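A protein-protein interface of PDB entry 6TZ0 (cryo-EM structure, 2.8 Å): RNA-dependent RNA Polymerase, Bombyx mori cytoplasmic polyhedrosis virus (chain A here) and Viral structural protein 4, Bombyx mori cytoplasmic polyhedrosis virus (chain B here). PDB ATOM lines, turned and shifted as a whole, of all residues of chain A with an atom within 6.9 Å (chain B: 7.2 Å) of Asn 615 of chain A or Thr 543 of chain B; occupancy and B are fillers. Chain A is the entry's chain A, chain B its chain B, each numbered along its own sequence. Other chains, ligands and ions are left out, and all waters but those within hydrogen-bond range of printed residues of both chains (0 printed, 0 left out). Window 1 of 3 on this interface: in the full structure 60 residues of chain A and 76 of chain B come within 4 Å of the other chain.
OG of Ser 616 of chain A is in hydrogen-bond range of O of Leu 541 of chain B. The backbone carbonyl oxygen (O) of Ala 614 of chain A lies close to the backbone carbonyl oxygen (O) of His 542 of chain B (3.0 Å). The guanidinium group (NH2) of Arg 377 of chain A sits at hydrogen-bond distance from the backbone carbonyl oxygen (O) of Thr 544 of chain B, 2.8 Å away. The backbone carbonyl oxygen of Ala 614 of chain A sits close to the backbone carbonyl oxygen of Leu 541 of chain B, at 3.4 Å.
The backbone carbonyl oxygen (O) of Thr 543 of chain B sits at hydrogen-bond distance from the backbone NH (N) of Leu 506 of chain B (2.9 Å). The backbone carbonyl oxygen (O) of Leu 611 of chain A is in hydrogen-bond range of the side-chain amide nitrogen (ND2) of Asn 615 of chain A.
NH1 of Arg 377 of chain A touches CE2 of Tyr 546 of chain B (3.3 Å). Phe 467 of chain A touches Gly 327 of chain B (CD1 to N, 3.3 Å). Ala 613 of chain A touches Leu 541 of chain B (O to CD2, 3.4 Å). O of Ala 614 of chain A touches O of Ala 540 of chain B (3.96 Å). O of Ala 614 of chain A touches N of Thr 543 of chain B, 3.8 Å away. OD1 of Asn 615 of chain A touches CG2 of Thr 543 of chain B, at 3.3 Å. His 542 of chain B touches Ser 616 of chain A (CD2 to O, 3.1 Å). OE1 of Gln 617 of chain A touches CG2 of Thr 504 of chain B, at 3.3 Å.
Of the printed residues of chain B, Arg 377 of chain A touches Thr 544 and Tyr 546. Of the printed residues of chain B, Phe 467 of chain A touches Gly 327 (3.3 Å). Of chain B, only Thr 543 comes within 4 Å of Asn 615 of chain A. Tyr 352 of chain B touches none of the printed residues of chain A. Of the printed residues of chain A, His 542 of chain B touches Ala 614 (3.0 Å) and Ser 616 (3.1 Å). Thr 543 of chain B touches two residues of chain A. The nearest residue of chain B that does not touch Asn 615 of chain A is Leu 541 of chain B (4.1 Å).
Of the 16 printed residues of chain A, 7 touch a printed residue of chain B. Hydrophobic or aromatic side chains of chain A that line the printed part of chain B: Phe 467. Printed residues of chain B that touch a printed residue of chain A: Gly 327, Thr 504, Ala 540, Leu 541, His 542, Thr 543, Thr 544 and Tyr 546. Among the printed residues, 12 pairs touch across the chains. Among the printed residues, no Asp or Glu carboxylate lies within 4 Å of a Lys or Arg side-chain nitrogen of the other chain.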
ATOM      1  N   ARG A 377       9.313   9.060   9.842  1.00  0.00           N
ATOM      2  CA  ARG A 377       9.262   8.408  11.146  1.00  0.00           C
ATOM      3  C   ARG A 377       9.399   6.896  11.045  1.00  0.00           C
ATOM      4  O   ARG A 377       9.142   6.209  12.037  1.00  0.00           O
ATOM      5  CB  ARG A 377       7.946   8.735  11.857  1.00  0.00           C
ATOM      6  CG  ARG A 377       7.646  10.210  12.080  1.00  0.00           C
ATOM      7  CD  ARG A 377       8.480  10.860  13.169  1.00  0.00           C
ATOM      8  NE  ARG A 377       8.204  10.299  14.486  1.00  0.00           N
ATOM      9  CZ  ARG A 377       8.918  10.565  15.574  1.00  0.00           C
ATOM     10  NH1 ARG A 377       9.933  11.411  15.509  1.00  0.00           N
ATOM     11  NH2 ARG A 377       8.608  10.004  16.730  1.00  0.00           N
ATOM     12  N   GLU A 379       7.434   4.940   9.506  1.00  0.00           N
ATOM     13  CA  GLU A 379       6.104   4.359   9.536  1.00  0.00           C
ATOM     14  C   GLU A 379       5.676   3.973   8.124  1.00  0.00           C
ATOM     15  O   GLU A 379       6.015   4.644   7.149  1.00  0.00           O
ATOM     16  CB  GLU A 379       5.124   5.357  10.142  1.00  0.00           C
ATOM     17  CG  GLU A 379       5.462   5.717  11.573  1.00  0.00           C
ATOM     18  CD  GLU A 379       4.625   6.857  12.104  1.00  0.00           C
ATOM     19  OE1 GLU A 379       3.865   7.461  11.323  1.00  0.00           O
ATOM     20  OE2 GLU A 379       4.733   7.159  13.309  1.00  0.00           O
ATOM     21  N   ILE A 466      -5.859  15.101  16.868  1.00  0.00           N
ATOM     22  CA  ILE A 466      -5.620  13.662  16.809  1.00  0.00           C
ATOM     23  C   ILE A 466      -4.636  13.233  17.894  1.00  0.00           C
ATOM     24  O   ILE A 466      -4.842  12.231  18.596  1.00  0.00           O
ATOM     25  CB  ILE A 466      -5.110  13.287  15.409  1.00  0.00           C
ATOM     26  CG1 ILE A 466      -6.076  13.793  14.331  1.00  0.00           C
ATOM     27  CG2 ILE A 466      -4.898  11.805  15.305  1.00  0.00           C
ATOM     28  CD1 ILE A 466      -7.471  13.237  14.425  1.00  0.00           C
ATOM     29  N   PHE A 467      -3.562  14.004  18.069  1.00  0.00           N
ATOM     30  CA  PHE A 467      -2.587  13.666  19.095  1.00  0.00           C
ATOM     31  C   PHE A 467      -3.143  13.918  20.485  1.00  0.00           C
ATOM     32  O   PHE A 467      -2.760  13.234  21.434  1.00  0.00           O
ATOM     33  CB  PHE A 467      -1.300  14.458  18.899  1.00  0.00           C
ATOM     34  CG  PHE A 467      -0.722  14.339  17.528  1.00  0.00           C
ATOM     35  CD1 PHE A 467      -0.308  13.119  17.038  1.00  0.00           C
ATOM     36  CD2 PHE A 467      -0.525  15.468  16.756  1.00  0.00           C
ATOM     37  CE1 PHE A 467       0.236  13.014  15.779  1.00  0.00           C
ATOM     38  CE2 PHE A 467       0.023  15.374  15.503  1.00  0.00           C
ATOM     39  CZ  PHE A 467       0.408  14.147  15.015  1.00  0.00           C
ATOM     40  N   LEU A 470      -4.987  10.788  21.281  1.00  0.00           N
ATOM     41  CA  LEU A 470      -4.132   9.658  21.654  1.00  0.00           C
ATOM     42  C   LEU A 470      -3.751   9.630  23.134  1.00  0.00           C
ATOM     43  O   LEU A 470      -3.135   8.656  23.575  1.00  0.00           O
ATOM     44  CB  LEU A 470      -2.850   9.650  20.826  1.00  0.00           C
ATOM     45  CG  LEU A 470      -2.962   9.279  19.353  1.00  0.00           C
ATOM     46  CD1 LEU A 470      -1.622   9.450  18.683  1.00  0.00           C
ATOM     47  CD2 LEU A 470      -3.454   7.862  19.224  1.00  0.00           C
ATOM     48  N   ARG A 496     -10.810   9.400  18.131  1.00  0.00           N
ATOM     49  CA  ARG A 496     -10.474   8.004  17.879  1.00  0.00           C
ATOM     50  C   ARG A 496     -11.495   7.341  16.972  1.00  0.00           C
ATOM     51  O   ARG A 496     -11.146   6.432  16.216  1.00  0.00           O
ATOM     52  CB  ARG A 496     -10.372   7.217  19.179  1.00  0.00           C
ATOM     53  CG  ARG A 496      -9.151   7.483  20.002  1.00  0.00           C
ATOM     54  CD  ARG A 496      -9.180   6.553  21.193  1.00  0.00           C
ATOM     55  NE  ARG A 496      -8.082   6.757  22.127  1.00  0.00           N
ATOM     56  CZ  ARG A 496      -6.916   6.130  22.046  1.00  0.00           C
ATOM     57  NH1 ARG A 496      -6.691   5.269  21.064  1.00  0.00           N
ATOM     58  NH2 ARG A 496      -5.975   6.365  22.948  1.00  0.00           N
ATOM     59  N   LEU A 499     -10.420   8.482  13.487  1.00  0.00           N
ATOM     60  CA  LEU A 499      -9.271   7.799  12.900  1.00  0.00           C
ATOM     61  C   LEU A 499      -9.666   6.488  12.235  1.00  0.00           C
ATOM     62  O   LEU A 499      -9.032   6.066  11.263  1.00  0.00           O
ATOM     63  CB  LEU A 499      -8.197   7.543  13.951  1.00  0.00           C
ATOM     64  CG  LEU A 499      -7.384   8.758  14.366  1.00  0.00           C
ATOM     65  CD1 LEU A 499      -6.408   8.364  15.455  1.00  0.00           C
ATOM     66  CD2 LEU A 499      -6.661   9.306  13.151  1.00  0.00           C
ATOM     67  N   ALA A 610      -2.371   5.888   7.180  1.00  0.00           N
ATOM     68  CA  ALA A 610      -1.049   5.529   7.674  1.00  0.00           C
ATOM     69  C   ALA A 610      -0.854   5.973   9.115  1.00  0.00           C
ATOM     70  O   ALA A 610      -0.232   5.258   9.910  1.00  0.00           O
ATOM     71  CB  ALA A 610       0.020   6.140   6.779  1.00  0.00           C
ATOM     72  N   LEU A 611      -1.399   7.137   9.479  1.00  0.00           N
ATOM     73  CA  LEU A 611      -1.281   7.598  10.853  1.00  0.00           C
ATOM     74  C   LEU A 611      -2.139   6.769  11.793  1.00  0.00           C
ATOM     75  O   LEU A 611      -1.768   6.577  12.955  1.00  0.00           O
ATOM     76  CB  LEU A 611      -1.642   9.082  10.930  1.00  0.00           C
ATOM     77  CG  LEU A 611      -1.333   9.860  12.209  1.00  0.00           C
ATOM     78  CD1 LEU A 611      -0.910  11.261  11.856  1.00  0.00           C
ATOM     79  CD2 LEU A 611      -2.527   9.928  13.131  1.00  0.00           C
ATOM     80  N   GLU A 612      -3.273   6.261  11.318  1.00  0.00           N
ATOM     81  CA  GLU A 612      -4.051   5.356  12.149  1.00  0.00           C
ATOM     82  C   GLU A 612      -3.355   4.012  12.302  1.00  0.00           C
ATOM     83  O   GLU A 612      -3.297   3.467  13.408  1.00  0.00           O
ATOM     84  CB  GLU A 612      -5.454   5.186  11.571  1.00  0.00           C
ATOM     85  CG  GLU A 612      -6.422   4.449  12.476  1.00  0.00           C
ATOM     86  CD  GLU A 612      -6.417   2.953  12.246  1.00  0.00           C
ATOM     87  OE1 GLU A 612      -6.186   2.532  11.097  1.00  0.00           O
ATOM     88  OE2 GLU A 612      -6.600   2.201  13.220  1.00  0.00           O
ATOM     89  N   ALA A 613      -2.828   3.457  11.209  1.00  0.00           N
ATOM     90  CA  ALA A 613      -2.191   2.149  11.265  1.00  0.00           C
ATOM     91  C   ALA A 613      -0.885   2.163  12.044  1.00  0.00           C
ATOM     92  O   ALA A 613      -0.490   1.124  12.576  1.00  0.00           O
ATOM     93  CB  ALA A 613      -1.940   1.629   9.854  1.00  0.00           C
ATOM     94  N   ALA A 614      -0.215   3.306  12.140  1.00  0.00           N
ATOM     95  CA  ALA A 614       1.047   3.367  12.857  1.00  0.00           C
ATOM     96  C   ALA A 614       0.895   3.687  14.336  1.00  0.00           C
ATOM     97  O   ALA A 614       1.863   3.535  15.084  1.00  0.00           O
ATOM     98  CB  ALA A 614       1.960   4.410  12.216  1.00  0.00           C
ATOM     99  N   ASN A 615      -0.277   4.137  14.776  1.00  0.00           N
ATOM    100  CA  ASN A 615      -0.508   4.532  16.164  1.00  0.00           C
ATOM    101  C   ASN A 615      -1.709   3.751  16.673  1.00  0.00           C
ATOM    102  O   ASN A 615      -2.831   4.257  16.683  1.00  0.00           O
ATOM    103  CB  ASN A 615      -0.752   6.028  16.254  1.00  0.00           C
ATOM    104  CG  ASN A 615       0.433   6.836  15.803  1.00  0.00           C
ATOM    105  OD1 ASN A 615       1.571   6.517  16.119  1.00  0.00           O
ATOM    106  ND2 ASN A 615       0.175   7.880  15.036  1.00  0.00           N
ATOM    107  N   SER A 616      -1.474   2.528  17.128  1.00  0.00           N
ATOM    108  CA  SER A 616      -2.553   1.606  17.455  1.00  0.00           C
ATOM    109  C   SER A 616      -2.508   1.264  18.934  1.00  0.00           C
ATOM    110  O   SER A 616      -1.497   0.753  19.427  1.00  0.00           O
ATOM    111  CB  SER A 616      -2.455   0.339  16.612  1.00  0.00           C
ATOM    112  OG  SER A 616      -1.280  -0.370  16.935  1.00  0.00           O
ATOM    113  N   GLN A 617      -3.600   1.541  19.636  1.00  0.00           N
ATOM    114  CA  GLN A 617      -3.726   1.201  21.046  1.00  0.00           C
ATOM    115  C   GLN A 617      -5.150   0.732  21.284  1.00  0.00           C
ATOM    116  O   GLN A 617      -6.096   1.503  21.110  1.00  0.00           O
ATOM    117  CB  GLN A 617      -3.404   2.397  21.939  1.00  0.00           C
ATOM    118  CG  GLN A 617      -3.299   2.029  23.388  1.00  0.00           C
ATOM    119  CD  GLN A 617      -2.051   1.241  23.676  1.00  0.00           C
ATOM    120  OE1 GLN A 617      -0.965   1.613  23.253  1.00  0.00           O
ATOM    121  NE2 GLN A 617      -2.199   0.133  24.381  1.00  0.00           N
ATOM    122  N   ARG A 641     -15.951   0.394  17.449  1.00  0.00           N
ATOM    123  CA  ARG A 641     -15.175   1.135  16.477  1.00  0.00           C
ATOM    124  C   ARG A 641     -15.984   1.249  15.184  1.00  0.00           C
ATOM    125  O   ARG A 641     -17.021   0.605  15.019  1.00  0.00           O
ATOM    126  CB  ARG A 641     -13.852   0.401  16.283  1.00  0.00           C
ATOM    127  CG  ARG A 641     -12.712   1.157  15.702  1.00  0.00           C
ATOM    128  CD  ARG A 641     -11.499   0.271  15.723  1.00  0.00           C
ATOM    129  NE  ARG A 641     -10.352   0.900  15.093  1.00  0.00           N
ATOM    130  CZ  ARG A 641      -9.174   0.312  14.957  1.00  0.00           C
ATOM    131  NH1 ARG A 641      -8.184   0.960  14.371  1.00  0.00           N
ATOM    132  NH2 ARG A 641      -8.989  -0.921  15.403  1.00  0.00           N
ATOM    133  N   GLY B 327       2.403  12.795  18.887  1.00  0.00           N
ATOM    134  CA  GLY B 327       1.864  11.531  19.355  1.00  0.00           C
ATOM    135  C   GLY B 327       2.764  10.833  20.347  1.00  0.00           C
ATOM    136  O   GLY B 327       2.279  10.177  21.275  1.00  0.00           O
ATOM    137  N   ALA B 328       4.079  10.976  20.171  1.00  0.00           N
ATOM    138  CA  ALA B 328       5.036  10.415  21.113  1.00  0.00           C
ATOM    139  C   ALA B 328       4.885  11.049  22.485  1.00  0.00           C
ATOM    140  O   ALA B 328       4.741  10.344  23.491  1.00  0.00           O
ATOM    141  CB  ALA B 328       6.453  10.610  20.584  1.00  0.00           C
ATOM    142  N   LEU B 329       4.881  12.385  22.537  1.00  0.00           N
ATOM    143  CA  LEU B 329       4.673  13.096  23.793  1.00  0.00           C
ATOM    144  C   LEU B 329       3.297  12.827  24.374  1.00  0.00           C
ATOM    145  O   LEU B 329       3.145  12.810  25.595  1.00  0.00           O
ATOM    146  CB  LEU B 329       4.855  14.597  23.594  1.00  0.00           C
ATOM    147  CG  LEU B 329       6.251  15.099  23.248  1.00  0.00           C
ATOM    148  CD1 LEU B 329       6.182  16.573  22.961  1.00  0.00           C
ATOM    149  CD2 LEU B 329       7.232  14.813  24.360  1.00  0.00           C
ATOM    150  N   VAL B 331       1.519   9.885  24.143  1.00  0.00           N
ATOM    151  CA  VAL B 331       1.503   8.571  24.782  1.00  0.00           C
ATOM    152  C   VAL B 331       2.397   8.562  26.023  1.00  0.00           C
ATOM    153  O   VAL B 331       2.055   7.965  27.057  1.00  0.00           O
ATOM    154  CB  VAL B 331       1.903   7.494  23.756  1.00  0.00           C
ATOM    155  CG1 VAL B 331       1.959   6.128  24.391  1.00  0.00           C
ATOM    156  CG2 VAL B 331       0.914   7.481  22.612  1.00  0.00           C
ATOM    157  N   LEU B 332       3.517   9.285  25.972  1.00  0.00           N
ATOM    158  CA  LEU B 332       4.390   9.365  27.138  1.00  0.00           C
ATOM    159  C   LEU B 332       3.757  10.165  28.275  1.00  0.00           C
ATOM    160  O   LEU B 332       3.917   9.814  29.448  1.00  0.00           O
ATOM    161  CB  LEU B 332       5.726   9.970  26.734  1.00  0.00           C
ATOM    162  CG  LEU B 332       6.606   9.110  25.836  1.00  0.00           C
ATOM    163  CD1 LEU B 332       7.750   9.938  25.333  1.00  0.00           C
ATOM    164  CD2 LEU B 332       7.102   7.895  26.585  1.00  0.00           C
ATOM    165  N   TYR B 352       9.035  -1.476  23.218  1.00  0.00           N
ATOM    166  CA  TYR B 352       9.565  -2.405  22.233  1.00  0.00           C
ATOM    167  C   TYR B 352      10.719  -1.772  21.473  1.00  0.00           C
ATOM    168  O   TYR B 352      10.724  -0.571  21.204  1.00  0.00           O
ATOM    169  CB  TYR B 352       8.500  -2.838  21.233  1.00  0.00           C
ATOM    170  CG  TYR B 352       7.399  -3.661  21.826  1.00  0.00           C
ATOM    171  CD1 TYR B 352       7.627  -4.965  22.208  1.00  0.00           C
ATOM    172  CD2 TYR B 352       6.118  -3.152  21.951  1.00  0.00           C
ATOM    173  CE1 TYR B 352       6.629  -5.727  22.742  1.00  0.00           C
ATOM    174  CE2 TYR B 352       5.107  -3.914  22.469  1.00  0.00           C
ATOM    175  CZ  TYR B 352       5.373  -5.203  22.866  1.00  0.00           C
ATOM    176  OH  TYR B 352       4.376  -5.980  23.389  1.00  0.00           O
ATOM    177  N   THR B 504       1.993   1.620  25.237  1.00  0.00           N
ATOM    178  CA  THR B 504       3.113   0.881  24.678  1.00  0.00           C
ATOM    179  C   THR B 504       3.677   1.639  23.486  1.00  0.00           C
ATOM    180  O   THR B 504       2.935   2.053  22.592  1.00  0.00           O
ATOM    181  CB  THR B 504       2.712  -0.560  24.311  1.00  0.00           C
ATOM    182  OG1 THR B 504       3.734  -1.173  23.517  1.00  0.00           O
ATOM    183  CG2 THR B 504       1.388  -0.632  23.620  1.00  0.00           C
ATOM    184  N   VAL B 505       4.988   1.857  23.512  1.00  0.00           N
ATOM    185  CA  VAL B 505       5.691   2.621  22.497  1.00  0.00           C
ATOM    186  C   VAL B 505       6.719   1.716  21.842  1.00  0.00           C
ATOM    187  O   VAL B 505       7.010   0.621  22.316  1.00  0.00           O
ATOM    188  CB  VAL B 505       6.369   3.876  23.070  1.00  0.00           C
ATOM    189  CG1 VAL B 505       5.345   4.803  23.655  1.00  0.00           C
ATOM    190  CG2 VAL B 505       7.393   3.490  24.113  1.00  0.00           C
ATOM    191  N   LEU B 506       7.282   2.200  20.742  1.00  0.00           N
ATOM    192  CA  LEU B 506       8.381   1.529  20.072  1.00  0.00           C
ATOM    193  C   LEU B 506       9.565   2.480  20.028  1.00  0.00           C
ATOM    194  O   LEU B 506       9.413   3.648  19.664  1.00  0.00           O
ATOM    195  CB  LEU B 506       7.977   1.076  18.669  1.00  0.00           C
ATOM    196  CG  LEU B 506       8.833   0.028  17.956  1.00  0.00           C
ATOM    197  CD1 LEU B 506       7.935  -0.835  17.115  1.00  0.00           C
ATOM    198  CD2 LEU B 506       9.875   0.650  17.072  1.00  0.00           C
ATOM    199  N   LEU B 507      10.734   1.972  20.388  1.00  0.00           N
ATOM    200  CA  LEU B 507      11.945   2.766  20.503  1.00  0.00           C
ATOM    201  C   LEU B 507      12.842   2.571  19.288  1.00  0.00           C
ATOM    202  O   LEU B 507      13.062   1.445  18.839  1.00  0.00           O
ATOM    203  CB  LEU B 507      12.681   2.385  21.790  1.00  0.00           C
ATOM    204  CG  LEU B 507      14.025   2.962  22.229  1.00  0.00           C
ATOM    205  CD1 LEU B 507      14.077   3.097  23.710  1.00  0.00           C
ATOM    206  CD2 LEU B 507      15.090   1.980  21.849  1.00  0.00           C
ATOM    207  N   ALA B 540       6.269  -1.701  12.926  1.00  0.00           N
ATOM    208  CA  ALA B 540       6.156  -0.407  13.593  1.00  0.00           C
ATOM    209  C   ALA B 540       4.692  -0.003  13.725  1.00  0.00           C
ATOM    210  O   ALA B 540       4.245   1.001  13.180  1.00  0.00           O
ATOM    211  CB  ALA B 540       6.953   0.646  12.832  1.00  0.00           C
ATOM    212  N   LEU B 541       3.938  -0.801  14.472  1.00  0.00           N
ATOM    213  CA  LEU B 541       2.505  -0.593  14.608  1.00  0.00           C
ATOM    214  C   LEU B 541       2.123   0.121  15.895  1.00  0.00           C
ATOM    215  O   LEU B 541       0.948   0.439  16.078  1.00  0.00           O
ATOM    216  CB  LEU B 541       1.768  -1.930  14.503  1.00  0.00           C
ATOM    217  CG  LEU B 541       1.895  -2.573  13.118  1.00  0.00           C
ATOM    218  CD1 LEU B 541       1.248  -3.933  13.044  1.00  0.00           C
ATOM    219  CD2 LEU B 541       1.321  -1.674  12.052  1.00  0.00           C
ATOM    220  N   HIS B 542       3.076   0.392  16.779  1.00  0.00           N
ATOM    221  CA  HIS B 542       2.867   1.289  17.903  1.00  0.00           C
ATOM    222  C   HIS B 542       3.601   2.596  17.652  1.00  0.00           C
ATOM    223  O   HIS B 542       4.336   2.732  16.671  1.00  0.00           O
ATOM    224  CB  HIS B 542       3.315   0.642  19.212  1.00  0.00           C
ATOM    225  CG  HIS B 542       2.471  -0.524  19.610  1.00  0.00           C
ATOM    226  ND1 HIS B 542       2.848  -1.829  19.390  1.00  0.00           N
ATOM    227  CD2 HIS B 542       1.226  -0.576  20.134  1.00  0.00           C
ATOM    228  CE1 HIS B 542       1.895  -2.636  19.816  1.00  0.00           C
ATOM    229  NE2 HIS B 542       0.897  -1.901  20.267  1.00  0.00           N
ATOM    230  N   THR B 543       3.379   3.569  18.534  1.00  0.00           N
ATOM    231  CA  THR B 543       3.908   4.908  18.311  1.00  0.00           C
ATOM    232  C   THR B 543       5.420   4.912  18.490  1.00  0.00           C
ATOM    233  O   THR B 543       5.942   4.375  19.467  1.00  0.00           O
ATOM    234  CB  THR B 543       3.273   5.913  19.269  1.00  0.00           C
ATOM    235  OG1 THR B 543       3.767   5.685  20.589  1.00  0.00           O
ATOM    236  CG2 THR B 543       1.782   5.737  19.293  1.00  0.00           C
ATOM    237  N   THR B 544       6.121   5.502  17.532  1.00  0.00           N
ATOM    238  CA  THR B 544       7.574   5.484  17.516  1.00  0.00           C
ATOM    239  C   THR B 544       8.111   6.655  18.325  1.00  0.00           C
ATOM    240  O   THR B 544       7.710   7.801  18.112  1.00  0.00           O
ATOM    241  CB  THR B 544       8.087   5.541  16.080  1.00  0.00           C
ATOM    242  OG1 THR B 544       7.587   4.411  15.358  1.00  0.00           O
ATOM    243  CG2 THR B 544       9.589   5.509  16.051  1.00  0.00           C
ATOM    244  N   VAL B 545       9.001   6.358  19.269  1.00  0.00           N
ATOM    245  CA  VAL B 545       9.539   7.342  20.198  1.00  0.00           C
ATOM    246  C   VAL B 545      11.059   7.238  20.166  1.00  0.00           C
ATOM    247  O   VAL B 545      11.605   6.131  20.182  1.00  0.00           O
ATOM    248  CB  VAL B 545       9.005   7.117  21.628  1.00  0.00           C
ATOM    249  CG1 VAL B 545       9.565   8.126  22.573  1.00  0.00           C
ATOM    250  CG2 VAL B 545       7.503   7.201  21.672  1.00  0.00           C
ATOM    251  N   TYR B 546      11.742   8.383  20.097  1.00  0.00           N
ATOM    252  CA  TYR B 546      13.188   8.478  20.218  1.00  0.00           C
ATOM    253  C   TYR B 546      13.578   8.768  21.663  1.00  0.00           C
ATOM    254  O   TYR B 546      12.736   9.187  22.459  1.00  0.00           O
ATOM    255  CB  TYR B 546      13.714   9.565  19.284  1.00  0.00           C
ATOM    256  CG  TYR B 546      13.598   9.207  17.829  1.00  0.00           C
ATOM    257  CD1 TYR B 546      14.397   8.220  17.277  1.00  0.00           C
ATOM    258  CD2 TYR B 546      12.736   9.893  16.996  1.00  0.00           C
ATOM    259  CE1 TYR B 546      14.301   7.892  15.952  1.00  0.00           C
ATOM    260  CE2 TYR B 546      12.643   9.579  15.664  1.00  0.00           C
ATOM    261  CZ  TYR B 546      13.428   8.580  15.145  1.00  0.00           C
ATOM    262  OH  TYR B 546      13.337   8.261  13.814  1.00  0.00           O
